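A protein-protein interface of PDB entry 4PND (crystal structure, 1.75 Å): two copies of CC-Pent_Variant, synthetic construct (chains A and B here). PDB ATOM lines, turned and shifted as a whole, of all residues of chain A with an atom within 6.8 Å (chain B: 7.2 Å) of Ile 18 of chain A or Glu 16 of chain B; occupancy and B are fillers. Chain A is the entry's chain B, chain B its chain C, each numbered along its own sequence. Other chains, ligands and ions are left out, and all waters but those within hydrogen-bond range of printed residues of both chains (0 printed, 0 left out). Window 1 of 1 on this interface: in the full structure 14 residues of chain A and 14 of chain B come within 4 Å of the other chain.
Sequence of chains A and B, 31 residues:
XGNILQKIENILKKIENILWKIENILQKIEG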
ATOM      1  N   ASN A  10      -1.516  17.431  -8.878  1.00  0.00           N
ATOM      2  CA  ASN A  10      -0.609  16.348  -9.260  1.00  0.00           C
ATOM      3  C   ASN A  10       0.788  16.514  -8.651  1.00  0.00           C
ATOM      4  O   ASN A  10       1.389  15.542  -8.193  1.00  0.00           O
ATOM      5  CB  ASN A  10      -0.500  16.271 -10.781  1.00  0.00           C
ATOM      6  CG  ASN A  10      -1.755  15.709 -11.419  1.00  0.00           C
ATOM      7  OD1 ASN A  10      -2.631  15.185 -10.724  1.00  0.00           O
ATOM      8  ND2 ASN A  10      -1.864  15.833 -12.747  1.00  0.00           N
ATOM      9  N   ILE A  11       1.300  17.740  -8.634  1.00  0.00           N
ATOM     10  CA  ILE A  11       2.622  18.005  -8.047  1.00  0.00           C
ATOM     11  C   ILE A  11       2.602  17.755  -6.532  1.00  0.00           C
ATOM     12  O   ILE A  11       3.556  17.203  -5.942  1.00  0.00           O
ATOM     13  CB  ILE A  11       3.080  19.452  -8.339  1.00  0.00           C
ATOM     14  CG1 ILE A  11       3.250  19.659  -9.843  1.00  0.00           C
ATOM     15  CG2 ILE A  11       4.417  19.736  -7.658  1.00  0.00           C
ATOM     16  CD1 ILE A  11       3.352  21.129 -10.261  1.00  0.00           C
ATOM     17  N   LEU A  12       1.504  18.140  -5.884  1.00  0.00           N
ATOM     18  CA  LEU A  12       1.386  17.914  -4.441  1.00  0.00           C
ATOM     19  C   LEU A  12       1.386  16.421  -4.112  1.00  0.00           C
ATOM     20  O   LEU A  12       1.987  16.009  -3.108  1.00  0.00           O
ATOM     21  CB  LEU A  12       0.116  18.583  -3.885  1.00  0.00           C
ATOM     22  CG  LEU A  12       0.178  20.102  -3.775  1.00  0.00           C
ATOM     23  CD1 LEU A  12      -1.228  20.681  -3.450  1.00  0.00           C
ATOM     24  CD2 LEU A  12       1.176  20.531  -2.709  1.00  0.00           C
ATOM     25  N   LYS A  13       0.743  15.612  -4.957  1.00  0.00           N
ATOM     26  CA  LYS A  13       0.760  14.151  -4.789  1.00  0.00           C
ATOM     27  C   LYS A  13       2.183  13.636  -4.899  1.00  0.00           C
ATOM     28  O   LYS A  13       2.576  12.737  -4.149  1.00  0.00           O
ATOM     29  CB  LYS A  13      -0.091  13.425  -5.833  1.00  0.00           C
ATOM     30  CG  LYS A  13      -1.587  13.506  -5.631  1.00  0.00           C
ATOM     31  CD  LYS A  13      -2.329  12.773  -6.735  1.00  0.00           C
ATOM     32  CE  LYS A  13      -3.817  12.685  -6.437  1.00  0.00           C
ATOM     33  NZ  LYS A  13      -4.561  11.956  -7.512  1.00  0.00           N
ATOM     34  N   LYS A  14       2.951  14.198  -5.833  1.00  0.00           N
ATOM     35  CA  LYS A  14       4.345  13.778  -6.011  1.00  0.00           C
ATOM     36  C   LYS A  14       5.182  14.166  -4.800  1.00  0.00           C
ATOM     37  O   LYS A  14       6.045  13.409  -4.347  1.00  0.00           O
ATOM     38  CB  LYS A  14       4.941  14.389  -7.279  1.00  0.00           C
ATOM     39  CG  LYS A  14       4.367  13.818  -8.571  1.00  0.00           C
ATOM     40  CD  LYS A  14       4.897  14.584  -9.781  1.00  0.00           C
ATOM     41  CE  LYS A  14       4.323  14.054 -11.100  1.00  0.00           C
ATOM     42  N   ILE A  15       4.939  15.364  -4.284  1.00  0.00           N
ATOM     43  CA  ILE A  15       5.612  15.826  -3.072  1.00  0.00           C
ATOM     44  C   ILE A  15       5.300  14.913  -1.883  1.00  0.00           C
ATOM     45  O   ILE A  15       6.195  14.577  -1.092  1.00  0.00           O
ATOM     46  CB  ILE A  15       5.215  17.290  -2.765  1.00  0.00           C
ATOM     47  CG1 ILE A  15       5.965  18.239  -3.716  1.00  0.00           C
ATOM     48  CG2 ILE A  15       5.497  17.634  -1.319  1.00  0.00           C
ATOM     49  CD1 ILE A  15       5.385  19.672  -3.745  1.00  0.00           C
ATOM     50  N   GLU A  16       4.036  14.517  -1.748  1.00  0.00           N
ATOM     51  CA  GLU A  16       3.644  13.594  -0.686  1.00  0.00           C
ATOM     52  C   GLU A  16       4.442  12.292  -0.802  1.00  0.00           C
ATOM     53  O   GLU A  16       4.988  11.785   0.182  1.00  0.00           O
ATOM     54  CB  GLU A  16       2.138  13.311  -0.737  1.00  0.00           C
ATOM     55  CG  GLU A  16       1.657  12.426   0.391  1.00  0.00           C
ATOM     56  CD  GLU A  16       0.242  11.913   0.178  1.00  0.00           C
ATOM     57  OE1 GLU A  16      -0.531  12.538  -0.582  1.00  0.00           O
ATOM     58  OE2 GLU A  16      -0.094  10.861   0.759  1.00  0.00           O
ATOM     59  N   ASN A  17       4.542  11.773  -2.021  1.00  0.00           N
ATOM     60  CA  ASN A  17       5.256  10.519  -2.228  1.00  0.00           C
ATOM     61  C   ASN A  17       6.733  10.628  -1.882  1.00  0.00           C
ATOM     62  O   ASN A  17       7.310   9.680  -1.325  1.00  0.00           O
ATOM     63  CB  ASN A  17       5.093  10.045  -3.668  1.00  0.00           C
ATOM     64  CG  ASN A  17       3.702   9.562  -3.942  1.00  0.00           C
ATOM     65  OD1 ASN A  17       3.011   9.125  -3.020  1.00  0.00           O
ATOM     66  ND2 ASN A  17       3.273   9.630  -5.203  1.00  0.00           N
ATOM     67  N   ILE A  18       7.350  11.749  -2.244  1.00  0.00           N
ATOM     68  CA  ILE A  18       8.770  11.946  -1.931  1.00  0.00           C
ATOM     69  C   ILE A  18       8.936  12.031  -0.415  1.00  0.00           C
ATOM     70  O   ILE A  18       9.879  11.490   0.151  1.00  0.00           O
ATOM     71  CB  ILE A  18       9.375  13.219  -2.573  1.00  0.00           C
ATOM     72  CG1 ILE A  18       9.247  13.191  -4.093  1.00  0.00           C
ATOM     73  CG2 ILE A  18      10.865  13.330  -2.192  1.00  0.00           C
ATOM     74  CD1 ILE A  18       9.470  14.563  -4.741  1.00  0.00           C
ATOM     75  N   LEU A  19       8.023  12.728   0.253  1.00  0.00           N
ATOM     76  CA  LEU A  19       8.108  12.847   1.717  1.00  0.00           C
ATOM     77  C   LEU A  19       7.940  11.485   2.401  1.00  0.00           C
ATOM     78  O   LEU A  19       8.550  11.229   3.445  1.00  0.00           O
ATOM     79  CB  LEU A  19       7.065  13.844   2.235  1.00  0.00           C
ATOM     80  CG  LEU A  19       7.448  15.300   1.970  1.00  0.00           C
ATOM     81  CD1 LEU A  19       6.255  16.218   2.272  1.00  0.00           C
ATOM     82  CD2 LEU A  19       8.655  15.698   2.833  1.00  0.00           C
ATOM     83  N   TRP A  20       7.078  10.623   1.859  1.00  0.00           N
ATOM     84  CA  TRP A  20       6.981   9.264   2.396  1.00  0.00           C
ATOM     85  C   TRP A  20       8.323   8.545   2.287  1.00  0.00           C
ATOM     86  O   TRP A  20       8.738   7.839   3.214  1.00  0.00           O
ATOM     87  CB  TRP A  20       5.918   8.432   1.659  1.00  0.00           C
ATOM     88  CG  TRP A  20       4.528   8.519   2.215  1.00  0.00           C
ATOM     89  CD1 TRP A  20       3.391   8.847   1.526  1.00  0.00           C
ATOM     90  CD2 TRP A  20       4.109   8.220   3.555  1.00  0.00           C
ATOM     91  NE1 TRP A  20       2.298   8.789   2.361  1.00  0.00           N
ATOM     92  CE2 TRP A  20       2.712   8.413   3.614  1.00  0.00           C
ATOM     93  CE3 TRP A  20       4.781   7.826   4.717  1.00  0.00           C
ATOM     94  CZ2 TRP A  20       1.975   8.225   4.785  1.00  0.00           C
ATOM     95  CZ3 TRP A  20       4.048   7.636   5.877  1.00  0.00           C
ATOM     96  CH2 TRP A  20       2.660   7.837   5.902  1.00  0.00           C
ATOM     97  N   LYS A  21       9.003   8.719   1.153  1.00  0.00           N
ATOM     98  CA  LYS A  21      10.307   8.066   0.969  1.00  0.00           C
ATOM     99  C   LYS A  21      11.314   8.596   1.970  1.00  0.00           C
ATOM    100  O   LYS A  21      12.068   7.830   2.577  1.00  0.00           O
ATOM    101  CB  LYS A  21      10.844   8.257  -0.458  1.00  0.00           C
ATOM    102  CG  LYS A  21      10.091   7.498  -1.548  1.00  0.00           C
ATOM    103  CD  LYS A  21      10.682   7.792  -2.934  1.00  0.00           C
ATOM    104  CE  LYS A  21      10.091   6.888  -4.003  1.00  0.00           C
ATOM    105  NZ  LYS A  21       8.608   6.839  -3.939  1.00  0.00           N
ATOM    106  N   ILE A  22      11.328   9.913   2.138  1.00  0.00           N
ATOM    107  CA  ILE A  22      12.215  10.540   3.123  1.00  0.00           C
ATOM    108  C   ILE A  22      11.909  10.034   4.534  1.00  0.00           C
ATOM    109  O   ILE A  22      12.817   9.702   5.312  1.00  0.00           O
ATOM    110  CB  ILE A  22      12.090  12.069   3.068  1.00  0.00           C
ATOM    111  CG1 ILE A  22      12.756  12.591   1.785  1.00  0.00           C
ATOM    112  CG2 ILE A  22      12.722  12.701   4.300  1.00  0.00           C
ATOM    113  CD1 ILE A  22      12.410  14.052   1.463  1.00  0.00           C
ATOM    114  N   GLU A  23      10.626   9.967   4.872  1.00  0.00           N
ATOM    115  CA  GLU A  23      10.236   9.483   6.191  1.00  0.00           C
ATOM    116  C   GLU A  23      10.698   8.052   6.426  1.00  0.00           C
ATOM    117  O   GLU A  23      11.181   7.720   7.519  1.00  0.00           O
ATOM    118  CB  GLU A  23       8.717   9.567   6.363  1.00  0.00           C
ATOM    119  CG  GLU A  23       8.223   9.356   7.784  1.00  0.00           C
ATOM    120  CD  GLU A  23       7.865   7.910   8.109  1.00  0.00           C
ATOM    121  OE1 GLU A  23       7.972   7.017   7.234  1.00  0.00           O
ATOM    122  OE2 GLU A  23       7.457   7.669   9.264  1.00  0.00           O
ATOM    123  N   ILE A  25      13.214   6.453   4.999  1.00  0.00           N
ATOM    124  CA  ILE A  25      14.673   6.448   5.107  1.00  0.00           C
ATOM    125  C   ILE A  25      15.090   6.904   6.500  1.00  0.00           C
ATOM    126  O   ILE A  25      15.983   6.312   7.103  1.00  0.00           O
ATOM    127  CB  ILE A  25      15.330   7.360   4.045  1.00  0.00           C
ATOM    128  CG1 ILE A  25      15.052   6.837   2.638  1.00  0.00           C
ATOM    129  CG2 ILE A  25      16.830   7.472   4.288  1.00  0.00           C
ATOM    130  CD1 ILE A  25      15.294   7.892   1.561  1.00  0.00           C
ATOM    131  N   ASN B  10       4.921  26.833 -10.347  1.00  0.00           N
ATOM    132  CA  ASN B  10       6.375  26.837 -10.519  1.00  0.00           C
ATOM    133  C   ASN B  10       7.108  26.645  -9.199  1.00  0.00           C
ATOM    134  O   ASN B  10       8.120  25.939  -9.136  1.00  0.00           O
ATOM    135  CB  ASN B  10       6.843  28.129 -11.183  1.00  0.00           C
ATOM    136  CG  ASN B  10       6.567  28.157 -12.681  1.00  0.00           C
ATOM    137  OD1 ASN B  10       6.226  27.135 -13.284  1.00  0.00           O
ATOM    138  ND2 ASN B  10       6.708  29.334 -13.286  1.00  0.00           N
ATOM    139  N   ILE B  11       6.608  27.270  -8.139  1.00  0.00           N
ATOM    140  CA  ILE B  11       7.239  27.103  -6.834  1.00  0.00           C
ATOM    141  C   ILE B  11       7.100  25.665  -6.339  1.00  0.00           C
ATOM    142  O   ILE B  11       8.030  25.114  -5.758  1.00  0.00           O
ATOM    143  CB  ILE B  11       6.661  28.069  -5.777  1.00  0.00           C
ATOM    144  CG1 ILE B  11       6.917  29.520  -6.187  1.00  0.00           C
ATOM    145  CG2 ILE B  11       7.294  27.802  -4.417  1.00  0.00           C
ATOM    146  CD1 ILE B  11       6.112  30.536  -5.397  1.00  0.00           C
ATOM    147  N   LEU B  12       5.944  25.053  -6.565  1.00  0.00           N
ATOM    148  CA  LEU B  12       5.744  23.655  -6.159  1.00  0.00           C
ATOM    149  C   LEU B  12       6.692  22.719  -6.911  1.00  0.00           C
ATOM    150  O   LEU B  12       7.190  21.748  -6.347  1.00  0.00           O
ATOM    151  CB  LEU B  12       4.292  23.228  -6.405  1.00  0.00           C
ATOM    152  CG  LEU B  12       3.269  23.856  -5.455  1.00  0.00           C
ATOM    153  CD1 LEU B  12       1.835  23.586  -5.941  1.00  0.00           C
ATOM    154  CD2 LEU B  12       3.442  23.320  -4.043  1.00  0.00           C
ATOM    155  N   LYS B  13       6.942  23.002  -8.188  1.00  0.00           N
ATOM    156  CA  LYS B  13       7.906  22.203  -8.942  1.00  0.00           C
ATOM    157  C   LYS B  13       9.309  22.313  -8.336  1.00  0.00           C
ATOM    158  O   LYS B  13      10.050  21.315  -8.260  1.00  0.00           O
ATOM    159  CB  LYS B  13       7.933  22.646 -10.401  1.00  0.00           C
ATOM    160  CG  LYS B  13       6.721  22.213 -11.215  1.00  0.00           C
ATOM    161  CD  LYS B  13       6.826  22.769 -12.630  1.00  0.00           C
ATOM    162  CE  LYS B  13       5.757  22.215 -13.549  1.00  0.00           C
ATOM    163  NZ  LYS B  13       5.883  22.781 -14.921  1.00  0.00           N
ATOM    164  N   LYS B  14       9.674  23.522  -7.904  1.00  0.00           N
ATOM    165  CA  LYS B  14      10.981  23.730  -7.258  1.00  0.00           C
ATOM    166  C   LYS B  14      11.052  23.004  -5.924  1.00  0.00           C
ATOM    167  O   LYS B  14      12.078  22.416  -5.582  1.00  0.00           O
ATOM    168  CB  LYS B  14      11.251  25.212  -7.040  1.00  0.00           C
ATOM    169  CG  LYS B  14      11.511  26.023  -8.317  1.00  0.00           C
ATOM    170  CD  LYS B  14      11.598  27.511  -7.987  1.00  0.00           C
ATOM    171  N   ILE B  15       9.965  23.055  -5.165  1.00  0.00           N
ATOM    172  CA  ILE B  15       9.880  22.334  -3.905  1.00  0.00           C
ATOM    173  C   ILE B  15      10.070  20.836  -4.132  1.00  0.00           C
ATOM    174  O   ILE B  15      10.830  20.192  -3.412  1.00  0.00           O
ATOM    175  CB  ILE B  15       8.528  22.612  -3.207  1.00  0.00           C
ATOM    176  CG1 ILE B  15       8.544  24.006  -2.570  1.00  0.00           C
ATOM    177  CG2 ILE B  15       8.225  21.547  -2.169  1.00  0.00           C
ATOM    178  CD1 ILE B  15       7.133  24.556  -2.202  1.00  0.00           C
ATOM    179  N   GLU B  16       9.402  20.301  -5.155  1.00  0.00           N
ATOM    180  CA  GLU B  16       9.526  18.892  -5.528  1.00  0.00           C
ATOM    181  C   GLU B  16      10.980  18.534  -5.840  1.00  0.00           C
ATOM    182  O   GLU B  16      11.517  17.518  -5.356  1.00  0.00           O
ATOM    183  CB  GLU B  16       8.614  18.597  -6.739  1.00  0.00           C
ATOM    184  CG  GLU B  16       8.545  17.142  -7.163  1.00  0.00           C
ATOM    185  CD  GLU B  16       7.858  16.931  -8.505  1.00  0.00           C
ATOM    186  OE1 GLU B  16       7.092  17.810  -8.951  1.00  0.00           O
ATOM    187  OE2 GLU B  16       8.067  15.863  -9.112  1.00  0.00           O
ATOM    188  N   ASN B  17      11.633  19.384  -6.630  1.00  0.00           N
ATOM    189  CA  ASN B  17      13.010  19.143  -7.032  1.00  0.00           C
ATOM    190  C   ASN B  17      13.968  19.154  -5.840  1.00  0.00           C
ATOM    191  O   ASN B  17      14.882  18.322  -5.748  1.00  0.00           O
ATOM    192  CB  ASN B  17      13.441  20.180  -8.069  1.00  0.00           C
ATOM    193  CG  ASN B  17      14.743  19.819  -8.744  1.00  0.00           C
ATOM    194  OD1 ASN B  17      14.792  18.902  -9.566  1.00  0.00           O
ATOM    195  ND2 ASN B  17      15.808  20.542  -8.407  1.00  0.00           N
ATOM    196  N   ILE B  18      13.759  20.085  -4.915  1.00  0.00           N
ATOM    197  CA  ILE B  18      14.608  20.149  -3.722  1.00  0.00           C
ATOM    198  C   ILE B  18      14.427  18.907  -2.851  1.00  0.00           C
ATOM    199  O   ILE B  18      15.395  18.349  -2.321  1.00  0.00           O
ATOM    200  CB  ILE B  18      14.314  21.415  -2.879  1.00  0.00           C
ATOM    201  CG1 ILE B  18      14.612  22.678  -3.692  1.00  0.00           C
ATOM    202  CG2 ILE B  18      15.154  21.418  -1.612  1.00  0.00           C
ATOM    203  CD1 ILE B  18      14.000  23.947  -3.093  1.00  0.00           C
ATOM    204  N   LEU B  19      13.182  18.467  -2.715  1.00  0.00           N
ATOM    205  CA  LEU B  19      12.872  17.283  -1.919  1.00  0.00           C
ATOM    206  C   LEU B  19      13.505  16.035  -2.520  1.00  0.00           C
ATOM    207  O   LEU B  19      13.998  15.168  -1.789  1.00  0.00           O
ATOM    208  CB  LEU B  19      11.358  17.110  -1.785  1.00  0.00           C
ATOM    209  CG  LEU B  19      10.680  18.073  -0.808  1.00  0.00           C
ATOM    210  CD1 LEU B  19       9.155  17.968  -0.982  1.00  0.00           C
ATOM    211  CD2 LEU B  19      11.059  17.740   0.641  1.00  0.00           C
ATOM    212  N   TRP B  20      13.518  15.941  -3.852  1.00  0.00           N
ATOM    213  CA  TRP B  20      14.208  14.829  -4.502  1.00  0.00           C
ATOM    214  C   TRP B  20      15.691  14.828  -4.142  1.00  0.00           C
ATOM    215  O   TRP B  20      16.277  13.765  -3.903  1.00  0.00           O
ATOM    216  CB  TRP B  20      14.057  14.881  -6.020  1.00  0.00           C
ATOM    217  CG  TRP B  20      12.850  14.158  -6.554  1.00  0.00           C
ATOM    218  CD1 TRP B  20      11.885  14.665  -7.391  1.00  0.00           C
ATOM    219  CD2 TRP B  20      12.486  12.794  -6.298  1.00  0.00           C
ATOM    220  NE1 TRP B  20      10.958  13.693  -7.680  1.00  0.00           N
ATOM    221  CE2 TRP B  20      11.294  12.544  -7.016  1.00  0.00           C
ATOM    222  CE3 TRP B  20      13.043  11.771  -5.522  1.00  0.00           C
ATOM    223  CZ2 TRP B  20      10.656  11.299  -6.986  1.00  0.00           C
ATOM    224  CZ3 TRP B  20      12.407  10.532  -5.501  1.00  0.00           C
ATOM    225  CH2 TRP B  20      11.225  10.313  -6.223  1.00  0.00           C
ATOM    226  N   LYS B  21      16.293  16.015  -4.104  1.00  0.00           N
ATOM    227  CA  LYS B  21      17.715  16.136  -3.758  1.00  0.00           C
ATOM    228  C   LYS B  21      17.969  15.684  -2.320  1.00  0.00           C
ATOM    229  O   LYS B  21      18.932  14.980  -2.042  1.00  0.00           O
ATOM    230  CB  LYS B  21      18.203  17.574  -3.930  1.00  0.00           C
ATOM    231  CG  LYS B  21      18.227  18.088  -5.367  1.00  0.00           C
ATOM    232  CD  LYS B  21      18.666  19.556  -5.402  1.00  0.00           C
ATOM    233  CE  LYS B  21      18.844  20.078  -6.818  1.00  0.00           C
ATOM    234  NZ  LYS B  21      18.972  18.970  -7.805  1.00  0.00           N
ATOM    235  N   ILE B  22      17.097  16.109  -1.413  1.00  0.00           N
ATOM    236  CA  ILE B  22      17.170  15.711  -0.006  1.00  0.00           C
ATOM    237  C   ILE B  22      17.027  14.188   0.113  1.00  0.00           C
ATOM    238  O   ILE B  22      17.796  13.529   0.799  1.00  0.00           O
ATOM    239  CB  ILE B  22      16.085  16.436   0.837  1.00  0.00           C
ATOM    240  CG1 ILE B  22      16.410  17.938   0.935  1.00  0.00           C
ATOM    241  CG2 ILE B  22      15.908  15.771   2.216  1.00  0.00           C
ATOM    242  CD1 ILE B  22      15.263  18.776   1.506  1.00  0.00           C
ATOM    243  N   GLU B  23      16.065  13.621  -0.599  1.00  0.00           N
ATOM    244  CA  GLU B  23      15.857  12.174  -0.582  1.00  0.00           C
ATOM    245  C   GLU B  23      17.092  11.438  -1.063  1.00  0.00           C
ATOM    246  O   GLU B  23      17.474  10.407  -0.496  1.00  0.00           O
ATOM    247  CB  GLU B  23      14.650  11.801  -1.453  1.00  0.00           C
ATOM    248  CG  GLU B  23      14.200  10.359  -1.298  1.00  0.00           C
ATOM    249  CD  GLU B  23      14.803   9.442  -2.334  1.00  0.00           C
ATOM    250  OE1 GLU B  23      15.528   9.931  -3.224  1.00  0.00           O
ATOM    251  OE2 GLU B  23      14.570   8.219  -2.252  1.00  0.00           O
ATOM    252  N   ASN B  24      17.727  11.956  -2.112  1.00  0.00           N
ATOM    253  CA  ASN B  24      18.900  11.275  -2.641  1.00  0.00           C
ATOM    254  C   ASN B  24      20.084  11.337  -1.680  1.00  0.00           C
ATOM    255  O   ASN B  24      20.825  10.355  -1.560  1.00  0.00           O
ATOM    256  CB  ASN B  24      19.312  11.831  -4.007  1.00  0.00           C
ATOM    257  CG  ASN B  24      20.403  10.989  -4.674  1.00  0.00           C
ATOM    258  OD1 ASN B  24      20.168   9.850  -5.100  1.00  0.00           O
ATOM    259  ND2 ASN B  24      21.598  11.554  -4.780  1.00  0.00           N
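Among the printed residues, pairs that only touch across the chains: Ile 18 of chain A with Trp 20 of chain B, Lys 14 of chain A with Glu 16 of chain B, Ile 11 of chain A with Glu 16 of chain B, Ile 18 of chain A with Glu 16 of chain B, Ile 18 of chain A with Leu 19 of chain B, Ile 11 of chain A with Lys 13 of chain B, Ile 11 of chain A with Leu 12 of chain B, Ile 15 of chain A with Leu 19 of chain B, Ile 15 of chain A with Ile 15 of chain B, Ile 15 of chain A with Leu 12 of chain B, Ile 22 of chain A with Leu 19 of chain B, Leu 12 of chain A with Leu 12 of chain B, Ile 22 of chain A with Glu 23 of chain B, Leu 19 of chain A with Leu 19 of chain B, Ile 25 of chain A with Glu 23 of chain B, Ile 22 of chain A with Ile 22 of chain B and Lys 21 of chain A with Glu 23 of chain B.
Ile 18 of chain A touches just these residues of chain B: Glu 16 (3.6 Å), Leu 19 (3.7 Å) and Trp 20 (3.4 Å). Glu 16 of chain B touches just these residues of chain A: Ile 11 (3.5 Å), Lys 14 (3.5 Å) and Ile 18 (3.6 Å). Of the printed residues of chain B, Ile 15 of chain A touches Leu 12 (3.8 Å), Ile 15 (3.8 Å) and Leu 19 (3.7 Å). Printed residues of chain A within 4 Å of Glu 23 of chain B: Lys 21 (3.97 Å), Ile 22 (3.8 Å) and Ile 25 (3.9 Å). Of the printed residues of chain A, Trp 20 of chain B touches Ile 18. Glu 23 of chain A touches none of the printed residues of chain B.
Hydrophobic or aromatic side chains of chain A that line the printed part of chain B: Ile 11, Leu 12, Ile 15, Ile 18, Leu 19, Ile 22 and Ile 25. Among the printed residues, 17 pairs touch across the chains. Among the printed residues, no Asp or Glu carboxylate lies within 4 Å of a Lys or Arg side-chain nitrogen of the other chain.
Lys 14 of chain A touches Glu 16 of chain B, but with the chains exchanged Glu 16 of chain A does not touch Lys 14 of chain B (11.8 Å). Ile 18 of chain A touches Trp 20 of chain B, but with the chains exchanged Trp 20 of chain A does not touch Ile 18 of chain B (12.0 Å). Lys 21 of chain A touches Glu 23 of chain B, but with the chains exchanged Glu 23 of chain A does not touch Lys 21 of chain B (11.8 Å). Ile 22 of chain A touches Leu 19 of chain B, but with the chains exchanged Leu 19 of chain A does not touch Ile 22 of chain B (7.3 Å). Of the 17 pairs that touch across the chains among the printed residues, 4 have their exchanged pair printed and touching as well.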
